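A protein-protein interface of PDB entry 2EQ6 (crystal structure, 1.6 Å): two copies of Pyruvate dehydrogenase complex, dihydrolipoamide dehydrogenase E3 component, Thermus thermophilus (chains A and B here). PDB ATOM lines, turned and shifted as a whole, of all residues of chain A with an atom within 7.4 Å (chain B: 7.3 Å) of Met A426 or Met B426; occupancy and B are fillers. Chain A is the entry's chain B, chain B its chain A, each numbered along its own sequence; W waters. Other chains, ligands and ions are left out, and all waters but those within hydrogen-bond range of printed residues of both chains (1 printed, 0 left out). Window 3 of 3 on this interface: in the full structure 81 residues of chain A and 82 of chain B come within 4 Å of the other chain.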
ATOM      1  N   LEU A 402       7.103  37.265 -30.081  1.00  0.00           N
ATOM      2  CA  LEU A 402       7.707  36.049 -30.625  1.00  0.00           C
ATOM      3  C   LEU A 402       8.985  36.332 -31.417  1.00  0.00           C
ATOM      4  O   LEU A 402       9.032  37.257 -32.227  1.00  0.00           O
ATOM      5  CB  LEU A 402       6.704  35.321 -31.530  1.00  0.00           C
ATOM      6  CG  LEU A 402       7.127  33.945 -32.057  1.00  0.00           C
ATOM      7  CD1 LEU A 402       7.228  32.962 -30.899  1.00  0.00           C
ATOM      8  CD2 LEU A 402       6.113  33.451 -33.080  1.00  0.00           C
ATOM      9  N   ALA A 420      20.215  30.680 -31.292  1.00  0.00           N
ATOM     10  CA  ALA A 420      19.060  31.272 -31.958  1.00  0.00           C
ATOM     11  C   ALA A 420      18.167  30.181 -32.548  1.00  0.00           C
ATOM     12  O   ALA A 420      16.940  30.263 -32.468  1.00  0.00           O
ATOM     13  CB  ALA A 420      19.518  32.229 -33.063  1.00  0.00           C
ATOM     14  N   ALA A 421      18.786  29.163 -33.143  1.00  0.00           N
ATOM     15  CA  ALA A 421      18.033  28.055 -33.731  1.00  0.00           C
ATOM     16  C   ALA A 421      17.223  27.343 -32.657  1.00  0.00           C
ATOM     17  O   ALA A 421      16.044  27.042 -32.850  1.00  0.00           O
ATOM     18  CB  ALA A 421      18.988  27.063 -34.415  1.00  0.00           C
ATOM     19  N   LEU A 422      17.856  27.071 -31.519  1.00  0.00           N
ATOM     20  CA  LEU A 422      17.163  26.404 -30.431  1.00  0.00           C
ATOM     21  C   LEU A 422      16.009  27.280 -29.951  1.00  0.00           C
ATOM     22  O   LEU A 422      14.920  26.782 -29.676  1.00  0.00           O
ATOM     23  CB  LEU A 422      18.125  26.140 -29.270  1.00  0.00           C
ATOM     24  CG  LEU A 422      17.484  25.638 -27.973  1.00  0.00           C
ATOM     25  CD1 LEU A 422      16.855  24.272 -28.192  1.00  0.00           C
ATOM     26  CD2 LEU A 422      18.543  25.569 -26.882  1.00  0.00           C
ATOM     27  N   ALA A 423      16.256  28.583 -29.852  1.00  0.00           N
ATOM     28  CA  ALA A 423      15.228  29.515 -29.400  1.00  0.00           C
ATOM     29  C   ALA A 423      14.001  29.402 -30.291  1.00  0.00           C
ATOM     30  O   ALA A 423      12.880  29.276 -29.801  1.00  0.00           O
ATOM     31  CB  ALA A 423      15.768  30.950 -29.412  1.00  0.00           C
ATOM     32  N   LEU A 424      14.210  29.429 -31.602  1.00  0.00           N
ATOM     33  CA  LEU A 424      13.092  29.317 -32.531  1.00  0.00           C
ATOM     34  C   LEU A 424      12.377  27.974 -32.393  1.00  0.00           C
ATOM     35  O   LEU A 424      11.145  27.915 -32.430  1.00  0.00           O
ATOM     36  CB  LEU A 424      13.576  29.502 -33.974  1.00  0.00           C
ATOM     37  CG  LEU A 424      14.130  30.881 -34.347  1.00  0.00           C
ATOM     38  CD1 LEU A 424      14.681  30.839 -35.766  1.00  0.00           C
ATOM     39  CD2 LEU A 424      13.036  31.939 -34.227  1.00  0.00           C
ATOM     40  N   GLU A 425      13.134  26.893 -32.232  1.00  0.00           N
ATOM     41  CA  GLU A 425      12.527  25.570 -32.098  1.00  0.00           C
ATOM     42  C   GLU A 425      11.701  25.455 -30.821  1.00  0.00           C
ATOM     43  O   GLU A 425      10.757  24.667 -30.756  1.00  0.00           O
ATOM     44  CB  GLU A 425      13.597  24.474 -32.104  1.00  0.00           C
ATOM     45  CG  GLU A 425      14.354  24.330 -33.417  1.00  0.00           C
ATOM     46  CD  GLU A 425      13.487  23.815 -34.554  1.00  0.00           C
ATOM     47  OE1 GLU A 425      12.309  23.470 -34.314  1.00  0.00           O
ATOM     48  OE2 GLU A 425      13.993  23.752 -35.690  1.00  0.00           O
ATOM     49  N   MET A 426      12.059  26.242 -29.807  1.00  0.00           N
ATOM     50  CA  MET A 426      11.344  26.220 -28.534  1.00  0.00           C
ATOM     51  C   MET A 426      10.232  27.264 -28.463  1.00  0.00           C
ATOM     52  O   MET A 426       9.557  27.380 -27.443  1.00  0.00           O
ATOM     53  CB  MET A 426      12.318  26.456 -27.375  1.00  0.00           C
ATOM     54  CG  MET A 426      13.401  25.397 -27.230  1.00  0.00           C
ATOM     55  SD  MET A 426      12.745  23.751 -26.943  1.00  0.00           S
ATOM     56  CE  MET A 426      12.099  23.906 -25.247  1.00  0.00           C
ATOM     57  N   GLY A 427      10.044  28.025 -29.538  1.00  0.00           N
ATOM     58  CA  GLY A 427       9.006  29.045 -29.544  1.00  0.00           C
ATOM     59  C   GLY A 427       9.316  30.187 -28.590  1.00  0.00           C
ATOM     60  O   GLY A 427       8.419  30.786 -27.990  1.00  0.00           O
ATOM     61  N   ALA A 428      10.600  30.504 -28.460  1.00  0.00           N
ATOM     62  CA  ALA A 428      11.041  31.568 -27.568  1.00  0.00           C
ATOM     63  C   ALA A 428      10.570  32.959 -27.972  1.00  0.00           C
ATOM     64  O   ALA A 428      10.374  33.251 -29.150  1.00  0.00           O
ATOM     65  CB  ALA A 428      12.564  31.562 -27.478  1.00  0.00           C
ATOM     66  N   THR A 429      10.383  33.811 -26.969  1.00  0.00           N
ATOM     67  CA  THR A 429       9.998  35.199 -27.191  1.00  0.00           C
ATOM     68  C   THR A 429      11.280  35.993 -26.994  1.00  0.00           C
ATOM     69  O   THR A 429      12.296  35.436 -26.565  1.00  0.00           O
ATOM     70  CB  THR A 429       8.994  35.689 -26.137  1.00  0.00           C
ATOM     71  OG1 THR A 429       9.568  35.530 -24.832  1.00  0.00           O
ATOM     72  CG2 THR A 429       7.697  34.901 -26.225  1.00  0.00           C
ATOM     73  N   ASP A 432      12.261  35.765 -23.512  1.00  0.00           N
ATOM     74  CA  ASP A 432      12.944  34.522 -23.150  1.00  0.00           C
ATOM     75  C   ASP A 432      14.433  34.641 -23.440  1.00  0.00           C
ATOM     76  O   ASP A 432      15.272  34.181 -22.662  1.00  0.00           O
ATOM     77  CB  ASP A 432      12.397  33.329 -23.943  1.00  0.00           C
ATOM     78  CG  ASP A 432      11.008  32.915 -23.507  1.00  0.00           C
ATOM     79  OD1 ASP A 432      10.728  32.928 -22.292  1.00  0.00           O
ATOM     80  OD2 ASP A 432      10.199  32.551 -24.386  1.00  0.00           O
ATOM     81  N   LEU A 433      14.758  35.254 -24.571  1.00  0.00           N
ATOM     82  CA  LEU A 433      16.145  35.425 -24.966  1.00  0.00           C
ATOM     83  C   LEU A 433      16.867  36.380 -24.021  1.00  0.00           C
ATOM     84  O   LEU A 433      17.997  36.125 -23.607  1.00  0.00           O
ATOM     85  CB  LEU A 433      16.217  35.947 -26.404  1.00  0.00           C
ATOM     86  CG  LEU A 433      17.610  36.099 -27.014  1.00  0.00           C
ATOM     87  CD1 LEU A 433      18.362  34.773 -26.901  1.00  0.00           C
ATOM     88  CD2 LEU A 433      17.482  36.524 -28.475  1.00  0.00           C
ATOM     89  N   THR A 436      17.612  34.916 -20.345  1.00  0.00           N
ATOM     90  CA  THR A 436      18.658  33.915 -20.168  1.00  0.00           C
ATOM     91  C   THR A 436      19.928  34.657 -19.753  1.00  0.00           C
ATOM     92  O   THR A 436      20.325  35.621 -20.403  1.00  0.00           O
ATOM     93  CB  THR A 436      18.923  33.144 -21.475  1.00  0.00           C
ATOM     94  OG1 THR A 436      17.745  32.415 -21.840  1.00  0.00           O
ATOM     95  CG2 THR A 436      20.087  32.169 -21.296  1.00  0.00           C
ATOM     96  N   LEU B 402      14.265  15.282 -19.324  1.00  0.00           N
ATOM     97  CA  LEU B 402      14.573  16.682 -19.048  1.00  0.00           C
ATOM     98  C   LEU B 402      16.075  16.947 -18.958  1.00  0.00           C
ATOM     99  O   LEU B 402      16.803  16.188 -18.329  1.00  0.00           O
ATOM    100  CB  LEU B 402      13.917  17.109 -17.734  1.00  0.00           C
ATOM    101  CG  LEU B 402      14.015  18.591 -17.369  1.00  0.00           C
ATOM    102  CD1 LEU B 402      13.140  19.409 -18.312  1.00  0.00           C
ATOM    103  CD2 LEU B 402      13.567  18.791 -15.926  1.00  0.00           C
ATOM    104  N   ALA B 420      23.052  26.174 -23.812  1.00  0.00           N
ATOM    105  CA  ALA B 420      22.644  25.276 -22.743  1.00  0.00           C
ATOM    106  C   ALA B 420      21.806  26.029 -21.712  1.00  0.00           C
ATOM    107  O   ALA B 420      20.805  25.506 -21.223  1.00  0.00           O
ATOM    108  CB  ALA B 420      23.874  24.654 -22.076  1.00  0.00           C
ATOM    109  N   ALA B 421      22.221  27.251 -21.382  1.00  0.00           N
ATOM    110  CA  ALA B 421      21.490  28.071 -20.414  1.00  0.00           C
ATOM    111  C   ALA B 421      20.077  28.331 -20.930  1.00  0.00           C
ATOM    112  O   ALA B 421      19.103  28.207 -20.188  1.00  0.00           O
ATOM    113  CB  ALA B 421      22.215  29.401 -20.180  1.00  0.00           C
ATOM    114  N   LEU B 422      19.968  28.689 -22.205  1.00  0.00           N
ATOM    115  CA  LEU B 422      18.658  28.944 -22.793  1.00  0.00           C
ATOM    116  C   LEU B 422      17.813  27.679 -22.734  1.00  0.00           C
ATOM    117  O   LEU B 422      16.624  27.726 -22.410  1.00  0.00           O
ATOM    118  CB  LEU B 422      18.808  29.396 -24.246  1.00  0.00           C
ATOM    119  CG  LEU B 422      17.500  29.549 -25.026  1.00  0.00           C
ATOM    120  CD1 LEU B 422      16.641  30.619 -24.368  1.00  0.00           C
ATOM    121  CD2 LEU B 422      17.805  29.913 -26.468  1.00  0.00           C
ATOM    122  N   ALA B 423      18.433  26.545 -23.048  1.00  0.00           N
ATOM    123  CA  ALA B 423      17.732  25.266 -23.035  1.00  0.00           C
ATOM    124  C   ALA B 423      17.113  25.020 -21.665  1.00  0.00           C
ATOM    125  O   ALA B 423      15.934  24.670 -21.553  1.00  0.00           O
ATOM    126  CB  ALA B 423      18.705  24.128 -23.390  1.00  0.00           C
ATOM    127  N   LEU B 424      17.907  25.206 -20.617  1.00  0.00           N
ATOM    128  CA  LEU B 424      17.418  25.004 -19.259  1.00  0.00           C
ATOM    129  C   LEU B 424      16.285  25.971 -18.909  1.00  0.00           C
ATOM    130  O   LEU B 424      15.290  25.574 -18.295  1.00  0.00           O
ATOM    131  CB  LEU B 424      18.563  25.163 -18.256  1.00  0.00           C
ATOM    132  CG  LEU B 424      19.665  24.102 -18.313  1.00  0.00           C
ATOM    133  CD1 LEU B 424      20.763  24.468 -17.323  1.00  0.00           C
ATOM    134  CD2 LEU B 424      19.089  22.727 -17.988  1.00  0.00           C
ATOM    135  N   GLU B 425      16.426  27.233 -19.301  1.00  0.00           N
ATOM    136  CA  GLU B 425      15.392  28.224 -19.001  1.00  0.00           C
ATOM    137  C   GLU B 425      14.077  27.894 -19.700  1.00  0.00           C
ATOM    138  O   GLU B 425      13.001  28.206 -19.187  1.00  0.00           O
ATOM    139  CB  GLU B 425      15.845  29.624 -19.420  1.00  0.00           C
ATOM    140  CG  GLU B 425      17.024  30.173 -18.622  1.00  0.00           C
ATOM    141  CD  GLU B 425      16.696  30.391 -17.155  1.00  0.00           C
ATOM    142  OE1 GLU B 425      17.609  30.767 -16.388  1.00  0.00           O
ATOM    143  OE2 GLU B 425      15.527  30.194 -16.765  1.00  0.00           O
ATOM    144  N   MET B 426      14.172  27.266 -20.869  1.00  0.00           N
ATOM    145  CA  MET B 426      12.998  26.897 -21.657  1.00  0.00           C
ATOM    146  C   MET B 426      12.438  25.525 -21.290  1.00  0.00           C
ATOM    147  O   MET B 426      11.447  25.084 -21.874  1.00  0.00           O
ATOM    148  CB  MET B 426      13.340  26.901 -23.150  1.00  0.00           C
ATOM    149  CG  MET B 426      13.758  28.249 -23.721  1.00  0.00           C
ATOM    150  SD  MET B 426      12.476  29.516 -23.631  1.00  0.00           S
ATOM    151  CE  MET B 426      11.269  28.888 -24.845  1.00  0.00           C
ATOM    152  N   GLY B 427      13.071  24.850 -20.334  1.00  0.00           N
ATOM    153  CA  GLY B 427      12.606  23.534 -19.930  1.00  0.00           C
ATOM    154  C   GLY B 427      12.803  22.492 -21.019  1.00  0.00           C
ATOM    155  O   GLY B 427      12.005  21.561 -21.164  1.00  0.00           O
ATOM    156  N   ALA B 428      13.880  22.640 -21.783  1.00  0.00           N
ATOM    157  CA  ALA B 428      14.177  21.714 -22.871  1.00  0.00           C
ATOM    158  C   ALA B 428      14.501  20.292 -22.422  1.00  0.00           C
ATOM    159  O   ALA B 428      15.024  20.068 -21.330  1.00  0.00           O
ATOM    160  CB  ALA B 428      15.339  22.257 -23.707  1.00  0.00           C
ATOM    161  N   THR B 429      14.176  19.332 -23.282  1.00  0.00           N
ATOM    162  CA  THR B 429      14.474  17.930 -23.026  1.00  0.00           C
ATOM    163  C   THR B 429      15.702  17.629 -23.876  1.00  0.00           C
ATOM    164  O   THR B 429      16.104  18.457 -24.699  1.00  0.00           O
ATOM    165  CB  THR B 429      13.340  17.005 -23.507  1.00  0.00           C
ATOM    166  OG1 THR B 429      13.132  17.205 -24.912  1.00  0.00           O
ATOM    167  CG2 THR B 429      12.046  17.302 -22.755  1.00  0.00           C
ATOM    168  N   ASP B 432      14.780  17.880 -27.416  1.00  0.00           N
ATOM    169  CA  ASP B 432      14.728  19.234 -27.965  1.00  0.00           C
ATOM    170  C   ASP B 432      16.106  19.679 -28.440  1.00  0.00           C
ATOM    171  O   ASP B 432      16.251  20.279 -29.505  1.00  0.00           O
ATOM    172  CB  ASP B 432      14.237  20.240 -26.919  1.00  0.00           C
ATOM    173  CG  ASP B 432      12.761  20.097 -26.612  1.00  0.00           C
ATOM    174  OD1 ASP B 432      11.970  19.932 -27.563  1.00  0.00           O
ATOM    175  OD2 ASP B 432      12.393  20.167 -25.420  1.00  0.00           O
ATOM    176  N   LEU B 433      17.115  19.398 -27.626  1.00  0.00           N
ATOM    177  CA  LEU B 433      18.483  19.775 -27.950  1.00  0.00           C
ATOM    178  C   LEU B 433      18.971  19.048 -29.201  1.00  0.00           C
ATOM    179  O   LEU B 433      19.599  19.644 -30.080  1.00  0.00           O
ATOM    180  CB  LEU B 433      19.395  19.455 -26.760  1.00  0.00           C
ATOM    181  CG  LEU B 433      20.869  19.847 -26.873  1.00  0.00           C
ATOM    182  CD1 LEU B 433      20.987  21.324 -27.236  1.00  0.00           C
ATOM    183  CD2 LEU B 433      21.569  19.558 -25.553  1.00  0.00           C
ATOM    184  N   THR B 436      17.325  20.304 -32.618  1.00  0.00           N
ATOM    185  CA  THR B 436      17.730  21.586 -33.179  1.00  0.00           C
ATOM    186  C   THR B 436      18.838  21.306 -34.188  1.00  0.00           C
ATOM    187  O   THR B 436      19.809  20.617 -33.873  1.00  0.00           O
ATOM    188  CB  THR B 436      18.259  22.533 -32.086  1.00  0.00           C
ATOM    189  OG1 THR B 436      17.190  22.853 -31.187  1.00  0.00           O
ATOM    190  CG2 THR B 436      18.807  23.816 -32.704  1.00  0.00           C
HETATM  191  O   HOH W   1      12.493  31.394 -20.557  1.00  0.00           O
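Leu A402 touches none of the printed residues of chain B. Met A426 touches just these residues of chain B: Met B426, Ala B428 and Asp B432. Of the printed residues of chain B, Thr A436 touches Ala B421, Leu B422 and Glu B425. Ala B420 touches none of the printed residues of chain A. Of the printed residues of chain A, Leu B422 touches Ala A423 (3.7 Å) and Thr A436 (3.3 Å). Met B426 touches just these residues of chain A: Met A426 (3.5 Å), Ala A428 (3.8 Å) and Asp A432 (3.7 Å). The nearest residue of chain A that does not touch Met B426 is Gly A427 (4.4 Å). The nearest printed residue of chain B that does not touch Ala A421 is Leu B422 (6.7 Å).
Leu A422 touches Thr B436, and with the chains exchanged Thr A436 touches Leu B422. Glu A425 touches Thr B436, and with the chains exchanged Thr A436 touches Glu B425. Met A426 touches its own counterpart, Met B426. Met A426 touches Ala B428, and with the chains exchanged Ala A428 touches Met B426.
Hydrophobic or aromatic side chains of chain A that line the printed part of chain B: Ala A421, Leu A422, Ala A423, Met A426 and Ala A428. Printed residues of chain B that touch a printed residue of chain A: Ala B421, Leu B422, Ala B423, Glu B425, Met B426, Ala B428, Asp B432 and Thr B436. Hydrophobic or aromatic side chains of chain B that line the printed part of chain A: Ala B421, Leu B422, Ala B423, Met B426 and Ala B428.
Water W1 bridges OD1 of Asp A432 (2.9 Å) and SD of Met B426 (3.6 Å).
Among the printed residues, merely in contact across the chains: Ala A421 with Thr B436, Leu A422 with Ala B423, Leu A422 with Thr B436, Ala A423 with Leu B422, Glu A425 with Thr B436, Met A426 with Met B426, Met A426 with Ala B428, Met A426 with Asp B432, Ala A428 with Met B426, Asp A432 with Met B426, Thr A436 with Ala B421, Thr A436 with Leu B422 and Thr A436 with Glu B425.
The backbone carbonyl oxygen (O) of Ala B423 lies within hydrogen-bond range of the backbone NH (N) of Ala B428 (2.9 Å). The backbone NH (N) of Thr B429 is in hydrogen-bond range of the side-chain carboxylate (OD2) of Asp B432, 2.9 Å away. The side-chain hydroxyl (OG1) of Thr B436 sits at hydrogen-bond distance from the backbone carbonyl oxygen (O) of Asp B432, at 3.2 Å. The backbone carbonyl oxygen of Ala A423 sits at hydrogen-bond distance from the backbone NH of Ala A428. OD2 of Asp A432 lies within hydrogen-bond range of N of Thr A429 (2.9 Å). O of Asp A432 lies within hydrogen-bond range of OG1 of Thr A436 (3.1 Å).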
